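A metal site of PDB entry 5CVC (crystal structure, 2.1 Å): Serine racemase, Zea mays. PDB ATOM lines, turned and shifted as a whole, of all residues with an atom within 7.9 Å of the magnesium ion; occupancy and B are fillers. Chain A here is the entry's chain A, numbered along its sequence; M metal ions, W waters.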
ATOM      1  N   ILE A 192      31.837 -18.388 -20.336  1.00  0.00           N
ATOM      2  CA  ILE A 192      30.526 -18.178 -19.719  1.00  0.00           C
ATOM      3  C   ILE A 192      29.417 -18.289 -20.744  1.00  0.00           C
ATOM      4  O   ILE A 192      29.540 -17.774 -21.863  1.00  0.00           O
ATOM      5  CB  ILE A 192      30.439 -16.870 -18.905  1.00  0.00           C
ATOM      6  CG1 ILE A 192      29.163 -16.823 -18.069  1.00  0.00           C
ATOM      7  CG2 ILE A 192      30.538 -15.638 -19.798  1.00  0.00           C
ATOM      8  CD1 ILE A 192      29.125 -15.725 -17.024  1.00  0.00           C
ATOM      9  N   SER A 193      28.357 -19.011 -20.389  1.00  0.00           N
ATOM     10  CA  SER A 193      27.155 -19.098 -21.199  1.00  0.00           C
ATOM     11  C   SER A 193      25.910 -18.927 -20.325  1.00  0.00           C
ATOM     12  O   SER A 193      25.272 -17.865 -20.367  1.00  0.00           O
ATOM     13  CB  SER A 193      27.094 -20.419 -21.970  1.00  0.00           C
ATOM     14  OG  SER A 193      26.027 -20.420 -22.926  1.00  0.00           O
ATOM     15  N   GLY A 194      25.520 -19.966 -19.600  1.00  0.00           N
ATOM     16  CA  GLY A 194      24.431 -19.855 -18.609  1.00  0.00           C
ATOM     17  C   GLY A 194      24.975 -19.437 -17.250  1.00  0.00           C
ATOM     18  O   GLY A 194      24.241 -18.900 -16.433  1.00  0.00           O
ATOM     19  N   ALA A 217      34.979 -15.101 -19.748  1.00  0.00           N
ATOM     20  CA  ALA A 217      35.329 -14.889 -21.147  1.00  0.00           C
ATOM     21  C   ALA A 217      34.084 -15.172 -21.987  1.00  0.00           C
ATOM     22  O   ALA A 217      33.483 -16.255 -21.880  1.00  0.00           O
ATOM     23  CB  ALA A 217      36.474 -15.792 -21.556  1.00  0.00           C
ATOM     24  N   GLU A 218      33.695 -14.205 -22.812  1.00  0.00           N
ATOM     25  CA  GLU A 218      32.404 -14.264 -23.506  1.00  0.00           C
ATOM     26  C   GLU A 218      32.513 -13.769 -24.948  1.00  0.00           C
ATOM     27  O   GLU A 218      33.228 -12.795 -25.224  1.00  0.00           O
ATOM     28  CB  GLU A 218      31.371 -13.408 -22.750  1.00  0.00           C
ATOM     29  CG  GLU A 218      29.935 -13.748 -23.124  1.00  0.00           C
ATOM     30  CD  GLU A 218      28.888 -12.927 -22.364  1.00  0.00           C
ATOM     31  OE1 GLU A 218      29.193 -11.776 -21.965  1.00  0.00           O
ATOM     32  OE2 GLU A 218      27.754 -13.440 -22.171  1.00  0.00           O
ATOM     33  N   PRO A 219      31.777 -14.409 -25.873  1.00  0.00           N
ATOM     34  CA  PRO A 219      31.806 -13.898 -27.256  1.00  0.00           C
ATOM     35  C   PRO A 219      31.096 -12.554 -27.439  1.00  0.00           C
ATOM     36  O   PRO A 219      30.066 -12.289 -26.820  1.00  0.00           O
ATOM     37  CB  PRO A 219      31.082 -14.978 -28.073  1.00  0.00           C
ATOM     38  CG  PRO A 219      30.949 -16.153 -27.171  1.00  0.00           C
ATOM     39  CD  PRO A 219      30.968 -15.632 -25.756  1.00  0.00           C
ATOM     40  N   LYS A 220      31.655 -11.731 -28.318  1.00  0.00           N
ATOM     41  CA  LYS A 220      31.068 -10.450 -28.694  1.00  0.00           C
ATOM     42  C   LYS A 220      29.637 -10.616 -29.205  1.00  0.00           C
ATOM     43  O   LYS A 220      28.779  -9.799 -28.904  1.00  0.00           O
ATOM     44  CB  LYS A 220      31.943  -9.783 -29.764  1.00  0.00           C
ATOM     45  CG  LYS A 220      31.517  -8.400 -30.187  1.00  0.00           C
ATOM     46  CD  LYS A 220      32.467  -7.847 -31.247  1.00  0.00           C
ATOM     47  N   GLY A 221      29.409 -11.674 -29.979  1.00  0.00           N
ATOM     48  CA  GLY A 221      28.104 -11.930 -30.562  1.00  0.00           C
ATOM     49  C   GLY A 221      27.130 -12.639 -29.618  1.00  0.00           C
ATOM     50  O   GLY A 221      26.067 -13.085 -30.041  1.00  0.00           O
ATOM     51  N   ALA A 222      27.506 -12.740 -28.341  1.00  0.00           N
ATOM     52  CA  ALA A 222      26.645 -13.332 -27.320  1.00  0.00           C
ATOM     53  C   ALA A 222      27.080 -12.824 -25.948  1.00  0.00           C
ATOM     54  O   ALA A 222      27.291 -13.608 -25.006  1.00  0.00           O
ATOM     55  CB  ALA A 222      26.718 -14.850 -27.393  1.00  0.00           C
ATOM     56  N   ASP A 223      27.163 -11.494 -25.852  1.00  0.00           N
ATOM     57  CA  ASP A 223      27.779 -10.781 -24.726  1.00  0.00           C
ATOM     58  C   ASP A 223      26.781 -10.324 -23.634  1.00  0.00           C
ATOM     59  O   ASP A 223      26.976  -9.288 -22.981  1.00  0.00           O
ATOM     60  CB  ASP A 223      28.530  -9.559 -25.246  1.00  0.00           C
ATOM     61  CG  ASP A 223      27.593  -8.480 -25.829  1.00  0.00           C
ATOM     62  OD1 ASP A 223      26.433  -8.796 -26.191  1.00  0.00           O
ATOM     63  OD2 ASP A 223      28.004  -7.314 -25.901  1.00  0.00           O
ATOM     64  N   ASP A 224      25.721 -11.098 -23.441  1.00  0.00           N
ATOM     65  CA  ASP A 224      24.683 -10.800 -22.442  1.00  0.00           C
ATOM     66  C   ASP A 224      25.160 -10.783 -20.985  1.00  0.00           C
ATOM     67  O   ASP A 224      24.601 -10.032 -20.165  1.00  0.00           O
ATOM     68  CB  ASP A 224      23.576 -11.849 -22.560  1.00  0.00           C
ATOM     69  CG  ASP A 224      24.101 -13.237 -22.407  1.00  0.00           C
ATOM     70  OD1 ASP A 224      24.800 -13.673 -23.331  1.00  0.00           O
ATOM     71  OD2 ASP A 224      23.848 -13.883 -21.370  1.00  0.00           O
ATOM     72  N   SER A 225      26.156 -11.605 -20.646  1.00  0.00           N
ATOM     73  CA  SER A 225      26.709 -11.595 -19.284  1.00  0.00           C
ATOM     74  C   SER A 225      27.413 -10.256 -18.982  1.00  0.00           C
ATOM     75  O   SER A 225      27.270  -9.690 -17.898  1.00  0.00           O
ATOM     76  CB  SER A 225      27.660 -12.781 -19.025  1.00  0.00           C
ATOM     77  OG  SER A 225      26.975 -14.026 -19.145  1.00  0.00           O
ATOM     78  N   ALA A 226      28.163  -9.761 -19.955  1.00  0.00           N
ATOM     79  CA  ALA A 226      28.829  -8.456 -19.848  1.00  0.00           C
ATOM     80  C   ALA A 226      27.758  -7.369 -19.762  1.00  0.00           C
ATOM     81  O   ALA A 226      27.853  -6.464 -18.944  1.00  0.00           O
ATOM     82  CB  ALA A 226      29.732  -8.207 -21.041  1.00  0.00           C
ATOM     83  N   GLN A 227      26.732  -7.483 -20.592  1.00  0.00           N
ATOM     84  CA  GLN A 227      25.647  -6.498 -20.546  1.00  0.00           C
ATOM     85  C   GLN A 227      24.931  -6.558 -19.224  1.00  0.00           C
ATOM     86  O   GLN A 227      24.636  -5.524 -18.651  1.00  0.00           O
ATOM     87  CB  GLN A 227      24.679  -6.671 -21.698  1.00  0.00           C
ATOM     88  CG  GLN A 227      25.344  -6.536 -23.054  1.00  0.00           C
ATOM     89  CD  GLN A 227      25.839  -5.129 -23.338  1.00  0.00           C
ATOM     90  OE1 GLN A 227      25.496  -4.182 -22.646  1.00  0.00           O
ATOM     91  NE2 GLN A 227      26.645  -4.997 -24.381  1.00  0.00           N
ATOM     92  N   ILE A 235      20.103  -9.463 -18.385  1.00  0.00           N
ATOM     93  CA  ILE A 235      19.753  -8.919 -19.681  1.00  0.00           C
ATOM     94  C   ILE A 235      19.878 -10.048 -20.696  1.00  0.00           C
ATOM     95  O   ILE A 235      20.786 -10.865 -20.582  1.00  0.00           O
ATOM     96  CB  ILE A 235      20.780  -7.804 -20.033  1.00  0.00           C
ATOM     97  CG1 ILE A 235      20.476  -6.514 -19.241  1.00  0.00           C
ATOM     98  CG2 ILE A 235      20.886  -7.576 -21.530  1.00  0.00           C
ATOM     99  CD1 ILE A 235      19.021  -6.119 -19.159  1.00  0.00           C
ATOM    100  N   LEU A 237      19.412 -11.082 -25.171  1.00  0.00           N
ATOM    101  CA  LEU A 237      19.616 -10.535 -26.506  1.00  0.00           C
ATOM    102  C   LEU A 237      18.551 -11.119 -27.425  1.00  0.00           C
ATOM    103  O   LEU A 237      18.071 -12.213 -27.184  1.00  0.00           O
ATOM    104  CB  LEU A 237      21.019 -10.866 -27.040  1.00  0.00           C
ATOM    105  CG  LEU A 237      22.204 -10.369 -26.205  1.00  0.00           C
ATOM    106  CD1 LEU A 237      23.511 -11.015 -26.640  1.00  0.00           C
ATOM    107  CD2 LEU A 237      22.289  -8.845 -26.256  1.00  0.00           C
ATOM    108  N   THR A 240      21.797 -14.382 -31.052  1.00  0.00           N
ATOM    109  CA  THR A 240      23.238 -14.448 -30.867  1.00  0.00           C
ATOM    110  C   THR A 240      23.908 -14.744 -32.198  1.00  0.00           C
ATOM    111  O   THR A 240      23.294 -15.204 -33.152  1.00  0.00           O
ATOM    112  CB  THR A 240      23.653 -15.508 -29.838  1.00  0.00           C
ATOM    113  OG1 THR A 240      23.394 -16.818 -30.355  1.00  0.00           O
ATOM    114  CG2 THR A 240      22.883 -15.316 -28.537  1.00  0.00           C
ATOM    115  N   THR A 242      27.642 -16.253 -32.806  1.00  0.00           N
ATOM    116  CA  THR A 242      28.989 -16.716 -32.523  1.00  0.00           C
ATOM    117  C   THR A 242      29.209 -18.154 -32.985  1.00  0.00           C
ATOM    118  O   THR A 242      28.311 -18.998 -32.923  1.00  0.00           O
ATOM    119  CB  THR A 242      29.356 -16.561 -31.028  1.00  0.00           C
ATOM    120  OG1 THR A 242      30.675 -17.088 -30.790  1.00  0.00           O
ATOM    121  CG2 THR A 242      28.347 -17.283 -30.135  1.00  0.00           C
ATOM    122  N   LEU A 247      28.220 -21.280 -26.115  1.00  0.00           N
ATOM    123  CA  LEU A 247      28.193 -20.017 -25.352  1.00  0.00           C
ATOM    124  C   LEU A 247      27.030 -19.091 -25.732  1.00  0.00           C
ATOM    125  O   LEU A 247      27.161 -17.873 -25.645  1.00  0.00           O
ATOM    126  CB  LEU A 247      29.541 -19.293 -25.447  1.00  0.00           C
ATOM    127  CG  LEU A 247      30.782 -20.150 -25.108  1.00  0.00           C
ATOM    128  CD1 LEU A 247      32.031 -19.309 -25.186  1.00  0.00           C
ATOM    129  CD2 LEU A 247      30.673 -20.818 -23.749  1.00  0.00           C
ATOM    130  N   ARG A 248      25.902 -19.675 -26.141  1.00  0.00           N
ATOM    131  CA  ARG A 248      24.779 -18.906 -26.670  1.00  0.00           C
ATOM    132  C   ARG A 248      23.601 -18.779 -25.695  1.00  0.00           C
ATOM    133  O   ARG A 248      22.564 -18.247 -26.075  1.00  0.00           O
ATOM    134  CB  ARG A 248      24.287 -19.535 -27.977  1.00  0.00           C
ATOM    135  CG  ARG A 248      25.294 -19.519 -29.103  1.00  0.00           C
ATOM    136  CD  ARG A 248      24.805 -20.400 -30.251  1.00  0.00           C
ATOM    137  NE  ARG A 248      25.699 -20.377 -31.393  1.00  0.00           N
ATOM    138  CZ  ARG A 248      25.820 -21.356 -32.305  1.00  0.00           C
ATOM    139  NH1 ARG A 248      25.121 -22.477 -32.202  1.00  0.00           N
ATOM    140  NH2 ARG A 248      26.681 -21.218 -33.299  1.00  0.00           N
ATOM    141  N   ALA A 249      23.746 -19.237 -24.470  1.00  0.00           N
ATOM    142  CA  ALA A 249      22.645 -19.173 -23.502  1.00  0.00           C
ATOM    143  C   ALA A 249      22.642 -17.845 -22.723  1.00  0.00           C
ATOM    144  O   ALA A 249      23.573 -17.031 -22.826  1.00  0.00           O
ATOM    145  CB  ALA A 249      22.724 -20.342 -22.547  1.00  0.00           C
ATOM    146  N   PHE A 250      21.611 -17.653 -21.914  1.00  0.00           N
ATOM    147  CA  PHE A 250      21.547 -16.502 -21.028  1.00  0.00           C
ATOM    148  C   PHE A 250      21.643 -16.963 -19.577  1.00  0.00           C
ATOM    149  O   PHE A 250      21.407 -18.120 -19.262  1.00  0.00           O
ATOM    150  CB  PHE A 250      20.279 -15.700 -21.297  1.00  0.00           C
ATOM    151  CG  PHE A 250      20.080 -15.347 -22.738  1.00  0.00           C
ATOM    152  CD1 PHE A 250      21.079 -14.729 -23.461  1.00  0.00           C
ATOM    153  CD2 PHE A 250      18.883 -15.614 -23.369  1.00  0.00           C
ATOM    154  CE1 PHE A 250      20.905 -14.404 -24.793  1.00  0.00           C
ATOM    155  CE2 PHE A 250      18.690 -15.274 -24.704  1.00  0.00           C
ATOM    156  CZ  PHE A 250      19.714 -14.675 -25.412  1.00  0.00           C
ATOM    157  N   LEU A 251      22.037 -16.046 -18.681  1.00  0.00           N
ATOM    158  CA  LEU A 251      22.154 -16.335 -17.262  1.00  0.00           C
ATOM    159  C   LEU A 251      20.821 -16.738 -16.646  1.00  0.00           C
ATOM    160  O   LEU A 251      19.770 -16.322 -17.112  1.00  0.00           O
ATOM    161  CB  LEU A 251      22.696 -15.104 -16.498  1.00  0.00           C
ATOM    162  CG  LEU A 251      24.065 -14.654 -16.979  1.00  0.00           C
ATOM    163  CD1 LEU A 251      24.468 -13.309 -16.391  1.00  0.00           C
ATOM    164  CD2 LEU A 251      25.110 -15.732 -16.700  1.00  0.00           C
ATOM    165  N   VAL A 266      33.885  -9.306 -17.133  1.00  0.00           N
ATOM    166  CA  VAL A 266      33.600 -10.160 -18.266  1.00  0.00           C
ATOM    167  C   VAL A 266      34.437  -9.673 -19.438  1.00  0.00           C
ATOM    168  O   VAL A 266      34.259  -8.558 -19.889  1.00  0.00           O
ATOM    169  CB  VAL A 266      32.112 -10.129 -18.634  1.00  0.00           C
ATOM    170  CG1 VAL A 266      31.849 -11.041 -19.812  1.00  0.00           C
ATOM    171  CG2 VAL A 266      31.280 -10.517 -17.428  1.00  0.00           C
HETATM  172 MG    MG M   1      26.585 -14.680 -23.292  1.00  0.00          MG
HETATM  173  O   HOH W   1      25.351 -16.002 -24.487  1.00  0.00           O
HETATM  174  O   HOH W   2      28.086 -16.324 -23.638  1.00  0.00           O
HETATM  175  O   HOH W   3      26.005 -15.537 -21.419  1.00  0.00           O
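OE1 of Glu 218 lies within hydrogen-bond range of N of Ala 226.
OE1 of Glu 218 lies within hydrogen-bond range of N of Ser 225, at 3.3 Å.
N of Ala 249 lies within hydrogen-bond range of OG of Ser 193, at 3.0 Å.
Ala 249 touches the magnesium ion (O to MG, 3.8 Å).
Four residues have an atom within 4 Å of the magnesium ion: Glu 218, Ala 222, Asp 224 and Ala 249.
Along chain A the residues within 4 Å of the magnesium ion span positions 218 to 249.
The nearest printed residue that does not touch the magnesium ion is Leu 247 (4.01 Å).
The magnesium ion is bound by OE2 of Glu 218 (2.0 Å), OD1 of Asp 224 (2.0 Å), water W3 (2.1 Å), O of Ala 222 (2.1 Å), water W1 (2.2 Å) and water W2 (2.3 Å).
Water W2 bridges O of Leu 247 (2.7 Å) and O of Ile 192 (2.7 Å).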
